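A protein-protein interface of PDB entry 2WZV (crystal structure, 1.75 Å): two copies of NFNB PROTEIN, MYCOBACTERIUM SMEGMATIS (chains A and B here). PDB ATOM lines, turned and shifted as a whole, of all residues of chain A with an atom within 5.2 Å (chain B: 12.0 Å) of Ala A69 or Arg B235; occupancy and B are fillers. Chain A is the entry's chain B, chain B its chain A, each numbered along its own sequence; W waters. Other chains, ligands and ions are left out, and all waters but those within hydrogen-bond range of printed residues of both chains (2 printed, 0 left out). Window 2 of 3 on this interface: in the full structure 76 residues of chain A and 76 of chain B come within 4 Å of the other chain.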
ATOM      1  N   GLU A  36      16.593 -21.150 -30.072  1.00  0.00           N
ATOM      2  CA  GLU A  36      15.887 -22.180 -29.317  1.00  0.00           C
ATOM      3  C   GLU A  36      14.386 -22.051 -29.411  1.00  0.00           C
ATOM      4  O   GLU A  36      13.844 -20.942 -29.511  1.00  0.00           O
ATOM      5  CB  GLU A  36      16.289 -22.151 -27.841  1.00  0.00           C
ATOM      6  CG  GLU A  36      17.738 -22.523 -27.586  1.00  0.00           C
ATOM      7  CD  GLU A  36      18.086 -22.519 -26.112  1.00  0.00           C
ATOM      8  OE1 GLU A  36      18.424 -23.600 -25.590  1.00  0.00           O
ATOM      9  OE2 GLU A  36      17.972 -21.452 -25.469  1.00  0.00           O
ATOM     10  N   GLU A  39      10.512 -22.713 -24.066  1.00  0.00           N
ATOM     11  CA  GLU A  39      10.189 -23.853 -23.207  1.00  0.00           C
ATOM     12  C   GLU A  39       8.699 -24.165 -23.142  1.00  0.00           C
ATOM     13  O   GLU A  39       8.346 -25.346 -23.149  1.00  0.00           O
ATOM     14  CB  GLU A  39      10.796 -23.713 -21.805  1.00  0.00           C
ATOM     15  CG  GLU A  39      12.289 -24.012 -21.795  1.00  0.00           C
ATOM     16  CD  GLU A  39      12.920 -24.081 -20.417  1.00  0.00           C
ATOM     17  OE1 GLU A  39      12.439 -24.878 -19.578  1.00  0.00           O
ATOM     18  OE2 GLU A  39      13.928 -23.374 -20.193  1.00  0.00           O
ATOM     19  N   MET A  42       7.786 -26.051 -26.340  1.00  0.00           N
ATOM     20  CA  MET A  42       8.257 -27.429 -26.247  1.00  0.00           C
ATOM     21  C   MET A  42       7.344 -28.249 -25.346  1.00  0.00           C
ATOM     22  O   MET A  42       6.985 -29.364 -25.712  1.00  0.00           O
ATOM     23  CB  MET A  42       9.699 -27.495 -25.748  1.00  0.00           C
ATOM     24  CG  MET A  42      10.663 -27.780 -26.871  1.00  0.00           C
ATOM     25  SD  MET A  42      12.480 -27.951 -26.272  1.00  0.00           S
ATOM     26  CE  MET A  42      12.650 -26.360 -25.258  1.00  0.00           C
ATOM     27  N   SER A  67      18.909 -30.051 -24.572  1.00  0.00           N
ATOM     28  CA  SER A  67      19.127 -28.667 -25.007  1.00  0.00           C
ATOM     29  C   SER A  67      20.387 -28.098 -24.347  1.00  0.00           C
ATOM     30  O   SER A  67      20.975 -28.747 -23.479  1.00  0.00           O
ATOM     31  CB  SER A  67      17.936 -27.799 -24.593  1.00  0.00           C
ATOM     32  OG  SER A  67      16.711 -28.320 -25.082  1.00  0.00           O
ATOM     33  N   GLY A  68      20.760 -26.879 -24.747  1.00  0.00           N
ATOM     34  CA  GLY A  68      21.873 -26.126 -24.177  1.00  0.00           C
ATOM     35  C   GLY A  68      23.193 -26.854 -24.056  1.00  0.00           C
ATOM     36  O   GLY A  68      23.578 -27.580 -24.969  1.00  0.00           O
ATOM     37  N   ALA A  69      23.918 -26.629 -22.932  1.00  0.00           N
ATOM     38  CA  ALA A  69      25.234 -27.247 -22.685  1.00  0.00           C
ATOM     39  C   ALA A  69      25.175 -28.784 -22.736  1.00  0.00           C
ATOM     40  O   ALA A  69      26.088 -29.384 -23.290  1.00  0.00           O
ATOM     41  CB  ALA A  69      25.806 -26.781 -21.354  1.00  0.00           C
ATOM     42  N   ALA A  70      24.101 -29.411 -22.209  1.00  0.00           N
ATOM     43  CA  ALA A  70      23.952 -30.874 -22.275  1.00  0.00           C
ATOM     44  C   ALA A  70      23.903 -31.332 -23.739  1.00  0.00           C
ATOM     45  O   ALA A  70      24.533 -32.337 -24.096  1.00  0.00           O
ATOM     46  CB  ALA A  70      22.688 -31.310 -21.554  1.00  0.00           C
ATOM     47  N   ARG A  71      23.179 -30.586 -24.590  1.00  0.00           N
ATOM     48  CA  ARG A  71      23.088 -30.881 -26.039  1.00  0.00           C
ATOM     49  C   ARG A  71      24.485 -30.738 -26.668  1.00  0.00           C
ATOM     50  O   ARG A  71      24.897 -31.585 -27.446  1.00  0.00           O
ATOM     51  CB  ARG A  71      22.022 -29.988 -26.708  1.00  0.00           C
ATOM     52  CG  ARG A  71      22.050 -29.887 -28.253  1.00  0.00           C
ATOM     53  CD  ARG A  71      22.745 -28.611 -28.756  1.00  0.00           C
ATOM     54  NE  ARG A  71      22.790 -28.599 -30.225  1.00  0.00           N
ATOM     55  CZ  ARG A  71      23.886 -28.758 -30.967  1.00  0.00           C
ATOM     56  NH1 ARG A  71      23.794 -28.804 -32.294  1.00  0.00           N
ATOM     57  NH2 ARG A  71      25.085 -28.854 -30.390  1.00  0.00           N
ATOM     58  N   ASP A  72      25.221 -29.679 -26.323  1.00  0.00           N
ATOM     59  CA  ASP A  72      26.589 -29.499 -26.812  1.00  0.00           C
ATOM     60  C   ASP A  72      27.502 -30.666 -26.407  1.00  0.00           C
ATOM     61  O   ASP A  72      28.239 -31.182 -27.260  1.00  0.00           O
ATOM     62  CB  ASP A  72      27.173 -28.172 -26.295  1.00  0.00           C
ATOM     63  CG  ASP A  72      26.496 -26.945 -26.873  1.00  0.00           C
ATOM     64  OD1 ASP A  72      26.645 -25.857 -26.281  1.00  0.00           O
ATOM     65  OD2 ASP A  72      25.800 -27.078 -27.907  1.00  0.00           O
ATOM     66  N   ARG A  73      27.451 -31.092 -25.116  1.00  0.00           N
ATOM     67  CA  ARG A  73      28.281 -32.219 -24.640  1.00  0.00           C
ATOM     68  C   ARG A  73      27.901 -33.518 -25.340  1.00  0.00           C
ATOM     69  O   ARG A  73      28.780 -34.302 -25.689  1.00  0.00           O
ATOM     70  CB  ARG A  73      28.160 -32.416 -23.123  1.00  0.00           C
ATOM     71  CG  ARG A  73      28.738 -31.269 -22.308  1.00  0.00           C
ATOM     72  CD  ARG A  73      28.859 -31.619 -20.827  1.00  0.00           C
ATOM     73  NE  ARG A  73      27.559 -31.850 -20.189  1.00  0.00           N
ATOM     74  CZ  ARG A  73      26.761 -30.899 -19.711  1.00  0.00           C
ATOM     75  NH1 ARG A  73      27.099 -29.620 -19.819  1.00  0.00           N
ATOM     76  NH2 ARG A  73      25.601 -31.218 -19.155  1.00  0.00           N
ATOM     77  N   LEU A  74      26.599 -33.730 -25.560  1.00  0.00           N
ATOM     78  CA  LEU A  74      26.080 -34.917 -26.224  1.00  0.00           C
ATOM     79  C   LEU A  74      26.576 -34.939 -27.685  1.00  0.00           C
ATOM     80  O   LEU A  74      27.091 -35.961 -28.121  1.00  0.00           O
ATOM     81  CB  LEU A  74      24.542 -34.939 -26.144  1.00  0.00           C
ATOM     82  CG  LEU A  74      23.868 -36.103 -26.874  1.00  0.00           C
ATOM     83  CD1 LEU A  74      24.371 -37.478 -26.350  1.00  0.00           C
ATOM     84  CD2 LEU A  74      22.358 -36.008 -26.718  1.00  0.00           C
ATOM     85  N   THR B 231       8.402 -38.139 -20.693  1.00  0.00           N
ATOM     86  CA  THR B 231       9.389 -37.235 -21.265  1.00  0.00           C
ATOM     87  C   THR B 231      10.271 -36.578 -20.214  1.00  0.00           C
ATOM     88  O   THR B 231       9.780 -36.084 -19.194  1.00  0.00           O
ATOM     89  CB  THR B 231       8.633 -36.186 -22.129  1.00  0.00           C
ATOM     90  OG1 THR B 231       7.680 -36.870 -22.936  1.00  0.00           O
ATOM     91  CG2 THR B 231       9.552 -35.343 -23.005  1.00  0.00           C
ATOM     92  N   ARG B 232      11.562 -36.512 -20.498  1.00  0.00           N
ATOM     93  CA  ARG B 232      12.508 -35.857 -19.596  1.00  0.00           C
ATOM     94  C   ARG B 232      13.275 -34.789 -20.366  1.00  0.00           C
ATOM     95  O   ARG B 232      13.834 -35.086 -21.425  1.00  0.00           O
ATOM     96  CB  ARG B 232      13.476 -36.897 -19.019  1.00  0.00           C
ATOM     97  CG  ARG B 232      14.627 -36.233 -18.238  1.00  0.00           C
ATOM     98  CD  ARG B 232      15.479 -37.222 -17.505  1.00  0.00           C
ATOM     99  NE  ARG B 232      16.565 -36.537 -16.803  1.00  0.00           N
ATOM    100  CZ  ARG B 232      17.847 -36.602 -17.143  1.00  0.00           C
ATOM    101  NH1 ARG B 232      18.228 -37.307 -18.203  1.00  0.00           N
ATOM    102  NH2 ARG B 232      18.762 -35.970 -16.418  1.00  0.00           N
ATOM    103  N   PHE B 233      13.292 -33.557 -19.841  1.00  0.00           N
ATOM    104  CA  PHE B 233      14.024 -32.444 -20.444  1.00  0.00           C
ATOM    105  C   PHE B 233      15.292 -32.153 -19.682  1.00  0.00           C
ATOM    106  O   PHE B 233      15.253 -31.980 -18.455  1.00  0.00           O
ATOM    107  CB  PHE B 233      13.155 -31.164 -20.490  1.00  0.00           C
ATOM    108  CG  PHE B 233      11.909 -31.286 -21.326  1.00  0.00           C
ATOM    109  CD1 PHE B 233      10.724 -31.780 -20.777  1.00  0.00           C
ATOM    110  CD2 PHE B 233      11.909 -30.899 -22.664  1.00  0.00           C
ATOM    111  CE1 PHE B 233       9.579 -31.926 -21.565  1.00  0.00           C
ATOM    112  CE2 PHE B 233      10.765 -31.040 -23.453  1.00  0.00           C
ATOM    113  CZ  PHE B 233       9.599 -31.531 -22.895  1.00  0.00           C
ATOM    114  N   SER B 234      16.424 -32.086 -20.385  1.00  0.00           N
ATOM    115  CA  SER B 234      17.665 -31.728 -19.703  1.00  0.00           C
ATOM    116  C   SER B 234      18.447 -30.693 -20.479  1.00  0.00           C
ATOM    117  O   SER B 234      18.302 -30.571 -21.700  1.00  0.00           O
ATOM    118  CB  SER B 234      18.509 -32.960 -19.405  1.00  0.00           C
ATOM    119  OG  SER B 234      19.024 -33.540 -20.588  1.00  0.00           O
ATOM    120  N   ARG B 235      19.260 -29.929 -19.743  1.00  0.00           N
ATOM    121  CA  ARG B 235      20.108 -28.884 -20.295  1.00  0.00           C
ATOM    122  C   ARG B 235      21.395 -28.717 -19.479  1.00  0.00           C
ATOM    123  O   ARG B 235      22.350 -28.106 -19.995  1.00  0.00           O
ATOM    124  CB  ARG B 235      19.355 -27.561 -20.569  1.00  0.00           C
ATOM    125  CG  ARG B 235      18.644 -26.910 -19.379  1.00  0.00           C
ATOM    126  CD  ARG B 235      17.535 -25.956 -19.827  1.00  0.00           C
ATOM    127  NE  ARG B 235      17.966 -25.065 -20.908  1.00  0.00           N
ATOM    128  CZ  ARG B 235      17.302 -24.862 -22.044  1.00  0.00           C
ATOM    129  NH1 ARG B 235      16.128 -25.450 -22.253  1.00  0.00           N
ATOM    130  NH2 ARG B 235      17.792 -24.051 -22.969  1.00  0.00           N
ATOM    131  OXT ARG B 235      21.464 -29.294 -18.366  1.00  0.00           O
HETATM  132  O   HOH W   1      15.650 -29.736 -23.056  1.00  0.00           O
HETATM  133  O   HOH W   2      22.645 -25.191 -20.641  1.00  0.00           O
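No position is printed for both chains.
Of the 5 printed residues of chain B, 2 touch a printed residue of chain A. Along chain B the printed residues that touch a printed residue of chain A span positions 234 to 235. Printed residues of chain A that touch a printed residue of chain B: Glu A36, Glu A39, Ser A67, Ala A69 and Ala A70. Hydrophobic or aromatic side chains of chain A within 4 Å of the printed part of chain B: Ala A69 and Ala A70. Among the printed residues, 6 pairs touch across the chains. Among the printed residues, Asp or Glu carboxylates within 4 Å of a Lys or Arg side-chain nitrogen of the other chain: Glu A36 with Arg B235 (2.7 Å) and Glu A39 with Arg B235 (3.7 Å).
Water W1 bridges the side-chain hydroxyl (OG) of Ser A67 (2.7 Å) and the backbone carbonyl oxygen (O) of Ser B234 (3.1 Å). Water W2 lies within hydrogen-bond range of N of Ala A69 (3.0 Å) and O of Arg B235 (3.0 Å).
Of the printed residues of chain B, Ala A69 touches Arg B235 (3.6 Å). Printed residues of chain A within 4 Å of Arg B235: Glu A36, Glu A39, Ser A67, Ala A69 and Ala A70. Asp A72 touches none of the printed residues of chain B. Printed residues of chain B within 4 Å of Ala A70: Arg B235. Printed residues of chain A within 4 Å of Ser B234: Ser A67. Leu A74 touches none of the printed residues of chain B.
O of Ser B234 sits at hydrogen-bond distance from N of Ser A67 (3.0 Å). The guanidinium group (NH2) of Arg B235 is in salt-bridge range of the side-chain carboxylate (OE1) of Glu A36, at 2.7 Å. The guanidinium group of Arg B235 lies within salt-bridge range of the side-chain carboxylate of Glu A39 (3.7 Å). O of Arg B235 is in hydrogen-bond range of N of Ala A70 (3.1 Å).
Among the printed residues, pairs that only touch across the chains: Ser A67 with Arg B235 and Ala A69 with Arg B235.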
